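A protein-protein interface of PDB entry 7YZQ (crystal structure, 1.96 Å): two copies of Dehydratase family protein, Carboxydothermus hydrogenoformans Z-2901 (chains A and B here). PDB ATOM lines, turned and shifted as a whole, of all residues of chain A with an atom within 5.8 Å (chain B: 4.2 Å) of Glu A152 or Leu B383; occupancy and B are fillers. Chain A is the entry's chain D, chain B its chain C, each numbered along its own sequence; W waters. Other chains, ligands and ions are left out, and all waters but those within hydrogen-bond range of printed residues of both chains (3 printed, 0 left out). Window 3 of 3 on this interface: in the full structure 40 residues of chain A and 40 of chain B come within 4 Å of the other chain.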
ATOM      1  N   LYS A 147     -23.067  -2.159  27.786  1.00  0.00           N
ATOM      2  CA  LYS A 147     -22.194  -2.408  26.640  1.00  0.00           C
ATOM      3  C   LYS A 147     -22.345  -1.315  25.604  1.00  0.00           C
ATOM      4  O   LYS A 147     -21.352  -0.789  25.081  1.00  0.00           O
ATOM      5  CB  LYS A 147     -22.509  -3.750  25.983  1.00  0.00           C
ATOM      6  CG  LYS A 147     -21.778  -4.953  26.561  1.00  0.00           C
ATOM      7  CD  LYS A 147     -22.432  -6.228  26.010  1.00  0.00           C
ATOM      8  CE  LYS A 147     -21.453  -7.271  25.615  1.00  0.00           C
ATOM      9  NZ  LYS A 147     -22.175  -8.517  25.210  1.00  0.00           N
ATOM     10  N   LYS A 148     -23.588  -0.978  25.287  1.00  0.00           N
ATOM     11  CA  LYS A 148     -23.836   0.036  24.269  1.00  0.00           C
ATOM     12  C   LYS A 148     -23.166   1.353  24.641  1.00  0.00           C
ATOM     13  O   LYS A 148     -22.573   2.009  23.785  1.00  0.00           O
ATOM     14  CB  LYS A 148     -25.339   0.246  24.075  1.00  0.00           C
ATOM     15  CG  LYS A 148     -25.681   1.515  23.259  1.00  0.00           C
ATOM     16  CD  LYS A 148     -27.165   1.619  22.954  1.00  0.00           C
ATOM     17  CE  LYS A 148     -28.027   1.648  24.230  1.00  0.00           C
ATOM     18  NZ  LYS A 148     -29.501   1.779  23.873  1.00  0.00           N
ATOM     19  N   LYS A 149     -23.270   1.781  25.901  1.00  0.00           N
ATOM     20  CA  LYS A 149     -22.667   3.059  26.270  1.00  0.00           C
ATOM     21  C   LYS A 149     -21.145   2.934  26.466  1.00  0.00           C
ATOM     22  O   LYS A 149     -20.393   3.900  26.266  1.00  0.00           O
ATOM     23  CB  LYS A 149     -23.348   3.587  27.539  1.00  0.00           C
ATOM     24  CG  LYS A 149     -24.838   3.887  27.426  1.00  0.00           C
ATOM     25  CD  LYS A 149     -25.239   4.692  26.206  1.00  0.00           C
ATOM     26  CE  LYS A 149     -24.911   6.151  26.356  1.00  0.00           C
ATOM     27  NZ  LYS A 149     -25.223   6.968  25.155  1.00  0.00           N
ATOM     28  N   ALA A 150     -20.670   1.754  26.855  1.00  0.00           N
ATOM     29  CA  ALA A 150     -19.232   1.543  27.006  1.00  0.00           C
ATOM     30  C   ALA A 150     -18.517   1.649  25.670  1.00  0.00           C
ATOM     31  O   ALA A 150     -17.366   2.109  25.626  1.00  0.00           O
ATOM     32  CB  ALA A 150     -18.921   0.163  27.613  1.00  0.00           C
ATOM     33  N   TRP A 151     -19.167   1.211  24.578  1.00  0.00           N
ATOM     34  CA  TRP A 151     -18.507   1.280  23.280  1.00  0.00           C
ATOM     35  C   TRP A 151     -18.079   2.701  22.969  1.00  0.00           C
ATOM     36  O   TRP A 151     -17.023   2.917  22.351  1.00  0.00           O
ATOM     37  CB  TRP A 151     -19.406   0.780  22.164  1.00  0.00           C
ATOM     38  CG  TRP A 151     -19.972  -0.589  22.357  1.00  0.00           C
ATOM     39  CD1 TRP A 151     -21.231  -0.997  22.008  1.00  0.00           C
ATOM     40  CD2 TRP A 151     -19.320  -1.736  22.916  1.00  0.00           C
ATOM     41  NE1 TRP A 151     -21.396  -2.328  22.329  1.00  0.00           N
ATOM     42  CE2 TRP A 151     -20.239  -2.802  22.880  1.00  0.00           C
ATOM     43  CE3 TRP A 151     -18.044  -1.978  23.410  1.00  0.00           C
ATOM     44  CZ2 TRP A 151     -19.926  -4.059  23.350  1.00  0.00           C
ATOM     45  CZ3 TRP A 151     -17.742  -3.221  23.888  1.00  0.00           C
ATOM     46  CH2 TRP A 151     -18.667  -4.254  23.846  1.00  0.00           C
ATOM     47  N   GLU A 152     -18.900   3.684  23.369  1.00  0.00           N
ATOM     48  CA  GLU A 152     -18.578   5.078  23.070  1.00  0.00           C
ATOM     49  C   GLU A 152     -17.278   5.485  23.766  1.00  0.00           C
ATOM     50  O   GLU A 152     -16.513   6.311  23.251  1.00  0.00           O
ATOM     51  CB  GLU A 152     -19.724   5.993  23.511  1.00  0.00           C
ATOM     52  CG  GLU A 152     -21.133   5.573  22.961  1.00  0.00           C
ATOM     53  CD  GLU A 152     -22.307   6.387  23.560  1.00  0.00           C
ATOM     54  OE1 GLU A 152     -22.090   7.189  24.471  1.00  0.00           O
ATOM     55  OE2 GLU A 152     -23.460   6.199  23.111  1.00  0.00           O
ATOM     56  N   ILE A 153     -17.034   4.933  24.947  1.00  0.00           N
ATOM     57  CA  ILE A 153     -15.789   5.199  25.664  1.00  0.00           C
ATOM     58  C   ILE A 153     -14.660   4.370  25.067  1.00  0.00           C
ATOM     59  O   ILE A 153     -13.532   4.850  24.927  1.00  0.00           O
ATOM     60  CB  ILE A 153     -15.978   4.886  27.160  1.00  0.00           C
ATOM     61  CG1 ILE A 153     -17.000   5.838  27.805  1.00  0.00           C
ATOM     62  CG2 ILE A 153     -14.662   4.936  27.900  1.00  0.00           C
ATOM     63  CD1 ILE A 153     -17.565   5.375  29.152  1.00  0.00           C
ATOM     64  N   LEU A 154     -14.948   3.115  24.701  1.00  0.00           N
ATOM     65  CA  LEU A 154     -13.904   2.228  24.203  1.00  0.00           C
ATOM     66  C   LEU A 154     -13.334   2.728  22.887  1.00  0.00           C
ATOM     67  O   LEU A 154     -12.150   2.512  22.600  1.00  0.00           O
ATOM     68  CB  LEU A 154     -14.451   0.815  24.050  1.00  0.00           C
ATOM     69  CG  LEU A 154     -13.454  -0.255  23.519  1.00  0.00           C
ATOM     70  CD1 LEU A 154     -12.264  -0.326  24.494  1.00  0.00           C
ATOM     71  CD2 LEU A 154     -14.120  -1.590  23.412  1.00  0.00           C
ATOM     72  N   ASN A 155     -14.144   3.426  22.097  1.00  0.00           N
ATOM     73  CA  ASN A 155     -13.676   3.918  20.809  1.00  0.00           C
ATOM     74  C   ASN A 155     -12.473   4.851  20.952  1.00  0.00           C
ATOM     75  O   ASN A 155     -11.711   5.020  19.996  1.00  0.00           O
ATOM     76  CB  ASN A 155     -14.819   4.625  20.084  1.00  0.00           C
ATOM     77  CG  ASN A 155     -14.489   4.950  18.622  1.00  0.00           C
ATOM     78  OD1 ASN A 155     -14.189   4.070  17.824  1.00  0.00           O
ATOM     79  ND2 ASN A 155     -14.527   6.243  18.285  1.00  0.00           N
ATOM     80  N   GLU A 156     -12.279   5.458  22.123  1.00  0.00           N
ATOM     81  CA  GLU A 156     -11.092   6.284  22.312  1.00  0.00           C
ATOM     82  C   GLU A 156      -9.813   5.472  22.351  1.00  0.00           C
ATOM     83  O   GLU A 156      -8.741   6.044  22.180  1.00  0.00           O
ATOM     84  CB  GLU A 156     -11.176   7.086  23.588  1.00  0.00           C
ATOM     85  CG  GLU A 156     -12.263   8.164  23.565  1.00  0.00           C
ATOM     86  CD  GLU A 156     -12.275   8.961  24.860  1.00  0.00           C
ATOM     87  OE1 GLU A 156     -13.126   9.870  24.983  1.00  0.00           O
ATOM     88  OE2 GLU A 156     -11.420   8.674  25.738  1.00  0.00           O
ATOM     89  N   PHE B 344     -29.915   6.399  23.145  1.00  0.00           N
ATOM     90  CA  PHE B 344     -29.332   6.495  21.809  1.00  0.00           C
ATOM     91  C   PHE B 344     -27.794   6.519  21.800  1.00  0.00           C
ATOM     92  O   PHE B 344     -27.133   7.000  22.734  1.00  0.00           O
ATOM     93  CB  PHE B 344     -29.873   7.757  21.127  1.00  0.00           C
ATOM     94  CG  PHE B 344     -31.296   7.620  20.711  1.00  0.00           C
ATOM     95  CD1 PHE B 344     -31.634   6.941  19.527  1.00  0.00           C
ATOM     96  CD2 PHE B 344     -32.302   8.069  21.525  1.00  0.00           C
ATOM     97  CE1 PHE B 344     -32.981   6.739  19.173  1.00  0.00           C
ATOM     98  CE2 PHE B 344     -33.663   7.880  21.163  1.00  0.00           C
ATOM     99  CZ  PHE B 344     -33.975   7.224  20.025  1.00  0.00           C
ATOM    100  N   THR B 345     -27.218   5.991  20.711  1.00  0.00           N
ATOM    101  CA  THR B 345     -25.773   5.988  20.546  1.00  0.00           C
ATOM    102  C   THR B 345     -25.412   6.408  19.128  1.00  0.00           C
ATOM    103  O   THR B 345     -26.063   5.953  18.164  1.00  0.00           O
ATOM    104  CB  THR B 345     -25.174   4.598  20.849  1.00  0.00           C
ATOM    105  OG1 THR B 345     -23.743   4.721  20.955  1.00  0.00           O
ATOM    106  CG2 THR B 345     -25.517   3.575  19.713  1.00  0.00           C
ATOM    107  N   PRO B 346     -24.448   7.341  18.954  1.00  0.00           N
ATOM    108  CA  PRO B 346     -23.890   8.162  20.041  1.00  0.00           C
ATOM    109  C   PRO B 346     -25.007   9.116  20.478  1.00  0.00           C
ATOM    110  O   PRO B 346     -26.087   9.153  19.863  1.00  0.00           O
ATOM    111  CB  PRO B 346     -22.767   8.913  19.372  1.00  0.00           C
ATOM    112  CG  PRO B 346     -23.324   9.197  18.016  1.00  0.00           C
ATOM    113  CD  PRO B 346     -24.189   7.976  17.639  1.00  0.00           C
ATOM    114  N   GLU B 380     -22.942   7.390  30.510  1.00  0.00           N
ATOM    115  CA  GLU B 380     -22.739   8.535  29.640  1.00  0.00           C
ATOM    116  C   GLU B 380     -22.199   9.722  30.410  1.00  0.00           C
ATOM    117  O   GLU B 380     -21.599  10.630  29.804  1.00  0.00           O
ATOM    118  CB  GLU B 380     -24.046   8.919  28.923  1.00  0.00           C
ATOM    119  CG  GLU B 380     -23.819  10.006  27.852  1.00  0.00           C
ATOM    120  CD  GLU B 380     -25.015  10.263  26.952  1.00  0.00           C
ATOM    121  OE1 GLU B 380     -25.293   9.375  26.120  1.00  0.00           O
ATOM    122  OE2 GLU B 380     -25.626  11.363  27.032  1.00  0.00           O
ATOM    123  N   SER B 381     -22.340   9.706  31.747  1.00  0.00           N
ATOM    124  CA  SER B 381     -21.869  10.857  32.530  1.00  0.00           C
ATOM    125  C   SER B 381     -20.348  11.051  32.430  1.00  0.00           C
ATOM    126  O   SER B 381     -19.852  12.176  32.569  1.00  0.00           O
ATOM    127  CB  SER B 381     -22.258  10.721  34.005  1.00  0.00           C
ATOM    128  OG  SER B 381     -21.535   9.649  34.615  1.00  0.00           O
ATOM    129  N   TYR B 382     -19.604   9.977  32.154  1.00  0.00           N
ATOM    130  CA  TYR B 382     -18.152  10.082  32.002  1.00  0.00           C
ATOM    131  C   TYR B 382     -17.771  11.018  30.869  1.00  0.00           C
ATOM    132  O   TYR B 382     -16.959  11.923  31.056  1.00  0.00           O
ATOM    133  CB  TYR B 382     -17.541   8.713  31.738  1.00  0.00           C
ATOM    134  CG  TYR B 382     -16.100   8.764  31.421  1.00  0.00           C
ATOM    135  CD1 TYR B 382     -15.161   9.100  32.422  1.00  0.00           C
ATOM    136  CD2 TYR B 382     -15.647   8.496  30.121  1.00  0.00           C
ATOM    137  CE1 TYR B 382     -13.780   9.140  32.124  1.00  0.00           C
ATOM    138  CE2 TYR B 382     -14.287   8.532  29.810  1.00  0.00           C
ATOM    139  CZ  TYR B 382     -13.360   8.873  30.801  1.00  0.00           C
ATOM    140  OH  TYR B 382     -12.036   8.931  30.468  1.00  0.00           O
ATOM    141  N   LEU B 383     -18.320  10.794  29.668  1.00  0.00           N
ATOM    142  CA  LEU B 383     -17.916  11.616  28.540  1.00  0.00           C
ATOM    143  C   LEU B 383     -18.497  13.006  28.658  1.00  0.00           C
ATOM    144  O   LEU B 383     -17.875  13.965  28.210  1.00  0.00           O
ATOM    145  CB  LEU B 383     -18.313  10.985  27.216  1.00  0.00           C
ATOM    146  CG  LEU B 383     -17.622   9.668  26.854  1.00  0.00           C
ATOM    147  CD1 LEU B 383     -18.473   8.938  25.728  1.00  0.00           C
ATOM    148  CD2 LEU B 383     -16.210   9.872  26.399  1.00  0.00           C
ATOM    149  N   VAL B 384     -19.651  13.162  29.298  1.00  0.00           N
ATOM    150  CA  VAL B 384     -20.177  14.509  29.486  1.00  0.00           C
ATOM    151  C   VAL B 384     -19.260  15.284  30.429  1.00  0.00           C
ATOM    152  O   VAL B 384     -18.856  16.412  30.146  1.00  0.00           O
ATOM    153  CB  VAL B 384     -21.621  14.453  30.017  1.00  0.00           C
ATOM    154  CG1 VAL B 384     -22.104  15.840  30.421  1.00  0.00           C
ATOM    155  CG2 VAL B 384     -22.544  13.828  28.978  1.00  0.00           C
ATOM    156  N   GLY B 385     -18.891  14.676  31.547  1.00  0.00           N
ATOM    157  CA  GLY B 385     -17.961  15.343  32.465  1.00  0.00           C
ATOM    158  C   GLY B 385     -16.629  15.706  31.820  1.00  0.00           C
ATOM    159  O   GLY B 385     -16.086  16.803  32.027  1.00  0.00           O
ATOM    160  N   ARG B 386     -16.070  14.766  31.055  1.00  0.00           N
ATOM    161  CA  ARG B 386     -14.823  15.013  30.357  1.00  0.00           C
ATOM    162  C   ARG B 386     -14.914  16.224  29.438  1.00  0.00           C
ATOM    163  O   ARG B 386     -13.985  17.015  29.384  1.00  0.00           O
ATOM    164  CB  ARG B 386     -14.423  13.783  29.559  1.00  0.00           C
ATOM    165  CG  ARG B 386     -13.983  12.613  30.418  1.00  0.00           C
ATOM    166  CD  ARG B 386     -12.479  12.415  30.339  1.00  0.00           C
ATOM    167  NE  ARG B 386     -12.057  12.227  28.964  1.00  0.00           N
ATOM    168  CZ  ARG B 386     -10.883  11.731  28.591  1.00  0.00           C
ATOM    169  NH1 ARG B 386     -10.593  11.602  27.290  1.00  0.00           N
ATOM    170  NH2 ARG B 386      -9.995  11.368  29.509  1.00  0.00           N
ATOM    171  N   GLU B 387     -16.003  16.380  28.686  1.00  0.00           N
ATOM    172  CA  GLU B 387     -16.081  17.538  27.801  1.00  0.00           C
ATOM    173  C   GLU B 387     -16.302  18.822  28.584  1.00  0.00           C
ATOM    174  O   GLU B 387     -15.689  19.847  28.274  1.00  0.00           O
ATOM    175  CB  GLU B 387     -17.169  17.345  26.758  1.00  0.00           C
ATOM    176  CG  GLU B 387     -17.335  18.543  25.780  1.00  0.00           C
ATOM    177  CD  GLU B 387     -16.179  18.711  24.802  1.00  0.00           C
ATOM    178  OE1 GLU B 387     -15.172  17.986  24.877  1.00  0.00           O
ATOM    179  OE2 GLU B 387     -16.275  19.591  23.940  1.00  0.00           O
HETATM  180  O   HOH W   1     -22.518   2.416  21.195  1.00  0.00           O
HETATM  181  O   HOH W   2     -11.456   7.411  28.233  1.00  0.00           O
HETATM  182  O   HOH W   3     -13.380  12.020  26.644  1.00  0.00           O
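Water W1 bridges OG1 of Thr B345 (2.6 Å) and O of Lys A148 (2.6 Å).
Water W3 bridges NE of Arg B386 (2.7 Å) and OE1 of Glu A156 (2.7 Å).
Water W2 bridges OH of Tyr B382 (2.8 Å) and OE2 of Glu A156 (2.8 Å).
The guanidinium group (NH2) of Arg B386 is in hydrogen-bond range of the side-chain hydroxyl (OH) of Tyr B382, at 3.3 Å.
The side-chain amino group of Lys A149 is in salt-bridge range of the side-chain carboxylate of Glu A152, at 2.8 Å.
No position is printed for both chains.
Of the printed residues of chain B, Lys A148 touches Thr B345.
Of chain B, only Phe B344 (3.8 Å), Thr B345 (2.6 Å), Pro B346 (3.7 Å) and Leu B383 (3.9 Å) come within 4 Å of Glu A152.
Of the printed residues of chain B, Ile A153 touches Tyr B382 (3.8 Å) and Leu B383 (3.995 Å).
Leu A154 touches none of the printed residues of chain B.
Asn A155 touches none of the printed residues of chain B.
Of the printed residues of chain A, Phe B344 touches Lys A149 and Glu A152.
Of the printed residues of chain A, Tyr B382 touches Ile A153.
Printed residues of chain A within 4 Å of Leu B383: Glu A152 (3.9 Å), Ile A153 (3.995 Å) and Glu A156 (3.4 Å).
Of the printed residues of chain A, Arg B386 touches Glu A156.
The nearest printed residue of chain B that does not touch Glu A152 is Glu B380 (4.2 Å).
NZ of Lys A149 lies within hydrogen-bond range of O of Phe B344, 3.1 Å away.
The side-chain hydroxyl of Thr B345 is in hydrogen-bond range of the side-chain carboxylate of Glu A152 (2.6 Å).
The side-chain carboxylate (OE1) of Glu B380 is in salt-bridge range of the side-chain amino group (NZ) of Lys A149 (2.6 Å).
NH1 of Arg B386 lies within salt-bridge range of OE2 of Glu A156 (3.4 Å).
Hydrophobic or aromatic side chains of chain B that line the printed part of chain A: Tyr B382 and Leu B383.
Along chain A the printed residues that touch a printed residue of chain B span positions 148 to 156.
Among the printed residues, merely in contact across the chains: Glu A156 with Leu B383 (3.4 Å), Glu A152 with Pro B346 (3.7 Å), Ile A153 with Tyr B382 (3.8 Å), Glu A152 with Phe B344 (3.8 Å), Glu A152 with Leu B383 (3.9 Å), Lys A148 with Thr B345 (3.9 Å) and Ile A153 with Leu B383 (3.995 Å).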
